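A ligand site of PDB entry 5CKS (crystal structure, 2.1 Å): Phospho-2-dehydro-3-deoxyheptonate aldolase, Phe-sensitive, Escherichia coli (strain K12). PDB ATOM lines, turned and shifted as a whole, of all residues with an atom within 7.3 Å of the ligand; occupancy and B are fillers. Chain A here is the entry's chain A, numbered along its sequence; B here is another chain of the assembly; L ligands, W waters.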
ATOM      1  N   PHE A  96       5.284  13.277  10.489  1.00  0.00           N
ATOM      2  CA  PHE A  96       4.196  13.807   9.675  1.00  0.00           C
ATOM      3  C   PHE A  96       3.711  12.822   8.613  1.00  0.00           C
ATOM      4  O   PHE A  96       2.734  13.081   7.916  1.00  0.00           O
ATOM      5  CB  PHE A  96       4.614  15.146   9.050  1.00  0.00           C
ATOM      6  CG  PHE A  96       4.934  16.191  10.073  1.00  0.00           C
ATOM      7  CD1 PHE A  96       3.914  16.793  10.804  1.00  0.00           C
ATOM      8  CD2 PHE A  96       6.242  16.570  10.323  1.00  0.00           C
ATOM      9  CE1 PHE A  96       4.204  17.757  11.758  1.00  0.00           C
ATOM     10  CE2 PHE A  96       6.526  17.527  11.266  1.00  0.00           C
ATOM     11  CZ  PHE A  96       5.499  18.130  11.982  1.00  0.00           C
ATOM     12  N   GLU A  97       4.395  11.691   8.501  1.00  0.00           N
ATOM     13  CA  GLU A  97       4.030  10.702   7.492  1.00  0.00           C
ATOM     14  C   GLU A  97       4.327   9.289   7.979  1.00  0.00           C
ATOM     15  O   GLU A  97       5.239   9.076   8.782  1.00  0.00           O
ATOM     16  CB  GLU A  97       4.790  10.983   6.186  1.00  0.00           C
ATOM     17  CG  GLU A  97       4.211  10.269   4.980  1.00  0.00           C
ATOM     18  CD  GLU A  97       4.995  10.530   3.694  1.00  0.00           C
ATOM     19  OE1 GLU A  97       5.634  11.605   3.571  1.00  0.00           O
ATOM     20  OE2 GLU A  97       4.986   9.652   2.805  1.00  0.00           O
ATOM     21  N   LYS A 106      -0.963  10.466   2.433  1.00  0.00           N
ATOM     22  CA  LYS A 106       0.415  10.847   2.227  1.00  0.00           C
ATOM     23  C   LYS A 106       0.987  11.678   3.374  1.00  0.00           C
ATOM     24  O   LYS A 106       2.136  12.112   3.307  1.00  0.00           O
ATOM     25  CB  LYS A 106       0.586  11.557   0.873  1.00  0.00           C
ATOM     26  CG  LYS A 106       0.595  10.600  -0.326  1.00  0.00           C
ATOM     27  CD  LYS A 106       1.913   9.849  -0.424  1.00  0.00           C
ATOM     28  CE  LYS A 106       3.058  10.791  -0.852  1.00  0.00           C
ATOM     29  NZ  LYS A 106       4.415  10.153  -0.785  1.00  0.00           N
ATOM     30  N   GLY A 107       0.198  11.908   4.414  1.00  0.00           N
ATOM     31  CA  GLY A 107       0.718  12.612   5.564  1.00  0.00           C
ATOM     32  C   GLY A 107       0.356  14.092   5.634  1.00  0.00           C
ATOM     33  O   GLY A 107      -0.243  14.643   4.707  1.00  0.00           O
ATOM     34  N   ILE A 109       2.205  16.949   5.800  1.00  0.00           N
ATOM     35  CA  ILE A 109       2.875  17.890   4.913  1.00  0.00           C
ATOM     36  C   ILE A 109       2.316  17.820   3.493  1.00  0.00           C
ATOM     37  O   ILE A 109       2.020  18.853   2.890  1.00  0.00           O
ATOM     38  CB  ILE A 109       4.396  17.695   4.956  1.00  0.00           C
ATOM     39  CG1 ILE A 109       4.902  18.008   6.370  1.00  0.00           C
ATOM     40  CG2 ILE A 109       5.071  18.569   3.926  1.00  0.00           C
ATOM     41  CD1 ILE A 109       6.371  17.656   6.631  1.00  0.00           C
ATOM     42  N   ASN A 110       2.146  16.614   2.975  1.00  0.00           N
ATOM     43  CA  ASN A 110       1.593  16.412   1.632  1.00  0.00           C
ATOM     44  C   ASN A 110       0.101  16.694   1.524  1.00  0.00           C
ATOM     45  O   ASN A 110      -0.368  17.301   0.565  1.00  0.00           O
ATOM     46  CB  ASN A 110       1.861  14.994   1.150  1.00  0.00           C
ATOM     47  CG  ASN A 110       3.320  14.736   0.878  1.00  0.00           C
ATOM     48  OD1 ASN A 110       3.987  15.539   0.244  1.00  0.00           O
ATOM     49  ND2 ASN A 110       3.828  13.609   1.377  1.00  0.00           N
ATOM     50  N   PHE A 118      -2.700  17.431  -2.344  1.00  0.00           N
ATOM     51  CA  PHE A 118      -1.303  17.881  -2.291  1.00  0.00           C
ATOM     52  C   PHE A 118      -1.130  19.376  -2.111  1.00  0.00           C
ATOM     53  O   PHE A 118      -0.717  20.080  -3.029  1.00  0.00           O
ATOM     54  CB  PHE A 118      -0.530  17.394  -3.511  1.00  0.00           C
ATOM     55  CG  PHE A 118      -0.295  15.921  -3.519  1.00  0.00           C
ATOM     56  CD1 PHE A 118       0.804  15.375  -2.858  1.00  0.00           C
ATOM     57  CD2 PHE A 118      -1.169  15.075  -4.182  1.00  0.00           C
ATOM     58  CE1 PHE A 118       1.027  14.002  -2.871  1.00  0.00           C
ATOM     59  CE2 PHE A 118      -0.949  13.710  -4.200  1.00  0.00           C
ATOM     60  CZ  PHE A 118       0.142  13.162  -3.542  1.00  0.00           C
ATOM     61  N   ILE A 120       1.137  21.175  -0.356  1.00  0.00           N
ATOM     62  CA  ILE A 120       2.378  21.046   0.367  1.00  0.00           C
ATOM     63  C   ILE A 120       2.829  22.338   1.032  1.00  0.00           C
ATOM     64  O   ILE A 120       3.349  22.307   2.141  1.00  0.00           O
ATOM     65  CB  ILE A 120       3.490  20.440  -0.512  1.00  0.00           C
ATOM     66  CG1 ILE A 120       3.048  19.048  -0.985  1.00  0.00           C
ATOM     67  CG2 ILE A 120       4.814  20.360   0.246  1.00  0.00           C
ATOM     68  CD1 ILE A 120       4.049  18.319  -1.852  1.00  0.00           C
ATOM     69  N   LEU A 124       3.510  22.379   4.979  1.00  0.00           N
ATOM     70  CA  LEU A 124       4.724  22.893   5.588  1.00  0.00           C
ATOM     71  C   LEU A 124       4.449  23.958   6.648  1.00  0.00           C
ATOM     72  O   LEU A 124       5.063  23.942   7.706  1.00  0.00           O
ATOM     73  CB  LEU A 124       5.672  23.435   4.509  1.00  0.00           C
ATOM     74  CG  LEU A 124       6.384  22.341   3.705  1.00  0.00           C
ATOM     75  CD1 LEU A 124       7.109  22.918   2.504  1.00  0.00           C
ATOM     76  CD2 LEU A 124       7.336  21.583   4.605  1.00  0.00           C
ATOM     77  N   LEU A 146      12.688  11.715   5.754  1.00  0.00           N
ATOM     78  CA  LEU A 146      12.426  10.817   4.638  1.00  0.00           C
ATOM     79  C   LEU A 146      13.029  11.327   3.323  1.00  0.00           C
ATOM     80  O   LEU A 146      13.242  10.556   2.394  1.00  0.00           O
ATOM     81  CB  LEU A 146      10.917  10.593   4.490  1.00  0.00           C
ATOM     82  CG  LEU A 146      10.224   9.947   5.701  1.00  0.00           C
ATOM     83  CD1 LEU A 146       8.704  10.014   5.576  1.00  0.00           C
ATOM     84  CD2 LEU A 146      10.687   8.492   5.887  1.00  0.00           C
ATOM     85  N   ASP A 147      13.321  12.622   3.269  1.00  0.00           N
ATOM     86  CA  ASP A 147      13.900  13.220   2.057  1.00  0.00           C
ATOM     87  C   ASP A 147      14.861  14.343   2.412  1.00  0.00           C
ATOM     88  O   ASP A 147      15.003  14.691   3.573  1.00  0.00           O
ATOM     89  CB  ASP A 147      12.796  13.760   1.160  1.00  0.00           C
ATOM     90  CG  ASP A 147      12.031  14.890   1.819  1.00  0.00           C
ATOM     91  OD1 ASP A 147      12.240  16.058   1.447  1.00  0.00           O
ATOM     92  OD2 ASP A 147      11.235  14.601   2.711  1.00  0.00           O
ATOM     93  N   MET A 148      15.501  14.911   1.393  1.00  0.00           N
ATOM     94  CA  MET A 148      16.560  15.884   1.613  1.00  0.00           C
ATOM     95  C   MET A 148      16.094  17.343   1.518  1.00  0.00           C
ATOM     96  O   MET A 148      16.895  18.259   1.716  1.00  0.00           O
ATOM     97  CB  MET A 148      17.735  15.658   0.638  1.00  0.00           C
ATOM     98  CG  MET A 148      18.782  14.625   1.118  1.00  0.00           C
ATOM     99  SD  MET A 148      18.050  12.991   1.278  1.00  0.00           S
ATOM    100  CE  MET A 148      17.409  12.807  -0.394  1.00  0.00           C
ATOM    101  N   ILE A 149      14.824  17.558   1.227  1.00  0.00           N
ATOM    102  CA  ILE A 149      14.325  18.933   1.123  1.00  0.00           C
ATOM    103  C   ILE A 149      13.478  19.394   2.325  1.00  0.00           C
ATOM    104  O   ILE A 149      13.699  20.472   2.865  1.00  0.00           O
ATOM    105  CB  ILE A 149      13.584  19.156  -0.205  1.00  0.00           C
ATOM    106  CG1 ILE A 149      14.559  18.979  -1.368  1.00  0.00           C
ATOM    107  CG2 ILE A 149      12.963  20.560  -0.255  1.00  0.00           C
ATOM    108  CD1 ILE A 149      13.909  19.043  -2.701  1.00  0.00           C
ATOM    109  N   THR A 150      12.516  18.571   2.726  1.00  0.00           N
ATOM    110  CA  THR A 150      11.770  18.784   3.969  1.00  0.00           C
ATOM    111  C   THR A 150      12.585  19.273   5.204  1.00  0.00           C
ATOM    112  O   THR A 150      12.157  20.220   5.865  1.00  0.00           O
ATOM    113  CB  THR A 150      10.960  17.523   4.346  1.00  0.00           C
ATOM    114  OG1 THR A 150      10.046  17.223   3.277  1.00  0.00           O
ATOM    115  CG2 THR A 150      10.166  17.755   5.619  1.00  0.00           C
ATOM    116  N   PRO A 151      13.744  18.656   5.509  1.00  0.00           N
ATOM    117  CA  PRO A 151      14.508  19.081   6.692  1.00  0.00           C
ATOM    118  C   PRO A 151      14.840  20.573   6.763  1.00  0.00           C
ATOM    119  O   PRO A 151      14.818  21.112   7.871  1.00  0.00           O
ATOM    120  CB  PRO A 151      15.788  18.260   6.589  1.00  0.00           C
ATOM    121  CG  PRO A 151      15.336  17.001   5.920  1.00  0.00           C
ATOM    122  CD  PRO A 151      14.349  17.464   4.884  1.00  0.00           C
ATOM    123  N   LEU A 154      12.217  22.384   8.864  1.00  0.00           N
ATOM    124  CA  LEU A 154      11.789  21.953  10.191  1.00  0.00           C
ATOM    125  C   LEU A 154      12.921  21.529  11.115  1.00  0.00           C
ATOM    126  O   LEU A 154      12.726  21.418  12.317  1.00  0.00           O
ATOM    127  CB  LEU A 154      10.812  20.786  10.051  1.00  0.00           C
ATOM    128  CG  LEU A 154       9.692  20.824   9.018  1.00  0.00           C
ATOM    129  CD1 LEU A 154       9.086  19.439   8.889  1.00  0.00           C
ATOM    130  CD2 LEU A 154       8.637  21.862   9.398  1.00  0.00           C
ATOM    131  N   GLN B 171      11.865   5.781  -1.328  1.00  0.00           N
ATOM    132  CA  GLN B 171      10.731   6.423  -1.990  1.00  0.00           C
ATOM    133  C   GLN B 171      11.123   7.595  -2.879  1.00  0.00           C
ATOM    134  O   GLN B 171      10.505   7.788  -3.915  1.00  0.00           O
ATOM    135  CB  GLN B 171       9.630   6.827  -0.998  1.00  0.00           C
ATOM    136  CG  GLN B 171       9.962   8.016  -0.097  1.00  0.00           C
ATOM    137  CD  GLN B 171       9.069   8.117   1.149  1.00  0.00           C
ATOM    138  OE1 GLN B 171       9.264   7.399   2.140  1.00  0.00           O
ATOM    139  NE2 GLN B 171       8.080   9.016   1.113  1.00  0.00           N
ATOM    140  N   VAL B 172      12.144   8.380  -2.503  1.00  0.00           N
ATOM    141  CA  VAL B 172      12.522   9.523  -3.336  1.00  0.00           C
ATOM    142  C   VAL B 172      13.164   9.038  -4.647  1.00  0.00           C
ATOM    143  O   VAL B 172      13.023   9.677  -5.696  1.00  0.00           O
ATOM    144  CB  VAL B 172      13.377  10.608  -2.593  1.00  0.00           C
ATOM    145  CG1 VAL B 172      12.618  11.197  -1.403  1.00  0.00           C
ATOM    146  CG2 VAL B 172      14.726  10.064  -2.148  1.00  0.00           C
ATOM    147  N   GLU B 175      10.231   7.864  -6.776  1.00  0.00           N
ATOM    148  CA  GLU B 175       9.628   9.075  -7.319  1.00  0.00           C
ATOM    149  C   GLU B 175      10.456   9.614  -8.482  1.00  0.00           C
ATOM    150  O   GLU B 175       9.905   9.966  -9.531  1.00  0.00           O
ATOM    151  CB  GLU B 175       9.472  10.150  -6.226  1.00  0.00           C
ATOM    152  CG  GLU B 175       8.420   9.806  -5.190  1.00  0.00           C
ATOM    153  CD  GLU B 175       8.556  10.600  -3.900  1.00  0.00           C
ATOM    154  OE1 GLU B 175       9.552  11.350  -3.720  1.00  0.00           O
ATOM    155  OE2 GLU B 175       7.660  10.460  -3.038  1.00  0.00           O
ATOM    156  N   HIS B 208       3.405  10.625  -9.220  1.00  0.00           N
ATOM    157  CA  HIS B 208       3.768  11.105  -7.911  1.00  0.00           C
ATOM    158  C   HIS B 208       3.788  12.619  -7.887  1.00  0.00           C
ATOM    159  O   HIS B 208       3.902  13.257  -8.911  1.00  0.00           O
ATOM    160  CB  HIS B 208       5.121  10.538  -7.489  1.00  0.00           C
ATOM    161  CG  HIS B 208       5.106   9.063  -7.281  1.00  0.00           C
ATOM    162  ND1 HIS B 208       4.855   8.484  -6.058  1.00  0.00           N
ATOM    163  CD2 HIS B 208       5.275   8.043  -8.158  1.00  0.00           C
ATOM    164  CE1 HIS B 208       4.875   7.176  -6.187  1.00  0.00           C
ATOM    165  NE2 HIS B 208       5.134   6.879  -7.452  1.00  0.00           N
ATOM    166  N   CYS B 209       3.662  13.167  -6.684  1.00  0.00           N
ATOM    167  CA  CYS B 209       3.804  14.597  -6.462  1.00  0.00           C
ATOM    168  C   CYS B 209       4.759  14.774  -5.294  1.00  0.00           C
ATOM    169  O   CYS B 209       4.507  14.267  -4.213  1.00  0.00           O
ATOM    170  CB  CYS B 209       2.446  15.210  -6.139  1.00  0.00           C
ATOM    171  SG  CYS B 209       2.533  16.942  -5.693  1.00  0.00           S
ATOM    172  N   PHE B 210       5.867  15.475  -5.493  1.00  0.00           N
ATOM    173  CA  PHE B 210       6.925  15.504  -4.483  1.00  0.00           C
ATOM    174  C   PHE B 210       7.852  16.686  -4.691  1.00  0.00           C
ATOM    175  O   PHE B 210       7.785  17.376  -5.721  1.00  0.00           O
ATOM    176  CB  PHE B 210       7.705  14.169  -4.517  1.00  0.00           C
ATOM    177  CG  PHE B 210       8.359  13.890  -5.862  1.00  0.00           C
ATOM    178  CD1 PHE B 210       9.670  14.269  -6.108  1.00  0.00           C
ATOM    179  CD2 PHE B 210       7.643  13.277  -6.878  1.00  0.00           C
ATOM    180  CE1 PHE B 210      10.254  14.048  -7.344  1.00  0.00           C
ATOM    181  CE2 PHE B 210       8.221  13.036  -8.107  1.00  0.00           C
ATOM    182  CZ  PHE B 210       9.536  13.431  -8.347  1.00  0.00           C
ATOM    183  N   LEU B 211       8.711  16.957  -3.714  1.00  0.00           N
ATOM    184  CA  LEU B 211       9.646  18.073  -3.815  1.00  0.00           C
ATOM    185  C   LEU B 211      10.899  17.732  -4.631  1.00  0.00           C
ATOM    186  O   LEU B 211      11.536  16.704  -4.398  1.00  0.00           O
ATOM    187  CB  LEU B 211      10.051  18.530  -2.418  1.00  0.00           C
ATOM    188  CG  LEU B 211       8.866  18.870  -1.526  1.00  0.00           C
ATOM    189  CD1 LEU B 211       9.359  19.460  -0.238  1.00  0.00           C
ATOM    190  CD2 LEU B 211       7.918  19.824  -2.246  1.00  0.00           C
ATOM    191  N   SER B 212      11.232  18.576  -5.602  1.00  0.00           N
ATOM    192  CA  SER B 212      12.431  18.354  -6.414  1.00  0.00           C
ATOM    193  C   SER B 212      13.076  19.674  -6.829  1.00  0.00           C
ATOM    194  O   SER B 212      12.694  20.740  -6.347  1.00  0.00           O
ATOM    195  CB  SER B 212      12.104  17.498  -7.637  1.00  0.00           C
ATOM    196  OG  SER B 212      13.287  17.116  -8.333  1.00  0.00           O
ATOM    197  N   ALA B 220      11.056  22.995  -6.032  1.00  0.00           N
ATOM    198  CA  ALA B 220       9.700  23.155  -6.510  1.00  0.00           C
ATOM    199  C   ALA B 220       8.885  21.917  -6.194  1.00  0.00           C
ATOM    200  O   ALA B 220       9.428  20.917  -5.753  1.00  0.00           O
ATOM    201  CB  ALA B 220       9.714  23.391  -8.001  1.00  0.00           C
HETATM  202  C1  LIG L   1       7.511  12.682   0.888  1.00  0.00           C
HETATM  203  C2  LIG L   1       8.125  12.584  -0.513  1.00  0.00           C
HETATM  204  C3  LIG L   1       9.315  13.515  -0.585  1.00  0.00           C
HETATM  205  C4  LIG L   1       8.854  14.942  -0.260  1.00  0.00           C
HETATM  206  C5  LIG L   1       8.192  14.946   1.117  1.00  0.00           C
HETATM  207  C6  LIG L   1       7.666  16.320   1.476  1.00  0.00           C
HETATM  208  O1  LIG L   1       6.401  11.822   0.972  1.00  0.00           O
HETATM  209  O2  LIG L   1       8.529  11.260  -0.757  1.00  0.00           O
HETATM  210  O3  LIG L   1       9.920  13.469  -1.849  1.00  0.00           O
HETATM  211  O4  LIG L   1       7.944  15.401  -1.250  1.00  0.00           O
HETATM  212  O5  LIG L   1       7.118  14.021   1.153  1.00  0.00           O
HETATM  213  O6  LIG L   1       7.457  16.321   2.880  1.00  0.00           O
HETATM  214  O   HOH W   1      12.003  15.152  -1.987  1.00  0.00           O
HETATM  215  O   HOH W   2       5.406  14.289  -1.727  1.00  0.00           O
HETATM  216  O   HOH W   3       6.143  14.181   4.397  1.00  0.00           O
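Water W1 lies within hydrogen-bond range of an oxygen (O3) of the ligand (2.7 Å) and the backbone carbonyl oxygen of Leu 211 of chain B (2.9 Å). Water W2 lies within hydrogen-bond range of O of Cys 209 of chain B, OD1 of Asn 110 and O4 of the ligand. Water W3 bridges OE1 of Glu 97 (2.8 Å) and O6 of the ligand (2.9 Å).
CG2 of Ile 109 touches O6 of the ligand, 3.4 Å away. Asp 147 touches the ligand. CG1 of Val 172 of chain B touches O3 of the ligand (3.6 Å). Phe 210 of chain B touches the ligand. 11 residues have an atom within 4 Å of the ligand: Glu 97, Lys 106, Ile 109, Asn 110, Asp 147, Thr 150, Gln 171 of chain B, Val 172 of chain B, Glu 175 of chain B, Phe 210 of chain B and Leu 211 of chain B. The nearest printed residue that does not touch the ligand is Cys 209 of chain B (4.7 Å).
The side-chain carboxylate (OE1) of Glu 97 is in hydrogen-bond range of the side-chain amide nitrogen (ND2) of Asn 110 (3.5 Å). The side-chain amino group (NZ) of Lys 106 lies within salt-bridge range of the side-chain carboxylate (OE2) of Glu 175 of chain B (3.96 Å). The side-chain carboxylate (OD1) of Asp 147 is in hydrogen-bond range of the backbone NH (N) of Ile 149, at 3.0 Å. N of Thr 150 sits at hydrogen-bond distance from OD1 of Asp 147 (2.8 Å). ND2 of Asn 110 lies within hydrogen-bond range of O of Lys 106, 3.0 Å away. The side-chain amino group (NZ) of Lys 106 lies within salt-bridge range of the side-chain carboxylate (OE2) of Glu 97 (3.7 Å).
OG1 of Thr 150 sits at hydrogen-bond distance from O6 of the ligand. The side-chain amino group (NZ) of Lys 106 lies within hydrogen-bond range of an oxygen (O1) of the ligand, 3.1 Å away. The side-chain amide nitrogen (NE2) of Gln 171 of chain B sits at hydrogen-bond distance from an oxygen (O2) of the ligand (3.0 Å). The side-chain carboxylate (OE1) of Glu 97 lies within hydrogen-bond range of an oxygen (O1) of the ligand (2.7 Å). The side-chain carboxylate (OE2) of Glu 175 of chain B sits at hydrogen-bond distance from an oxygen (O2) of the ligand (2.6 Å). N of Leu 211 of chain B is in hydrogen-bond range of O4 of the ligand (3.0 Å). ND2 of Asn 110 is in hydrogen-bond range of O1 of the ligand, at 3.2 Å.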
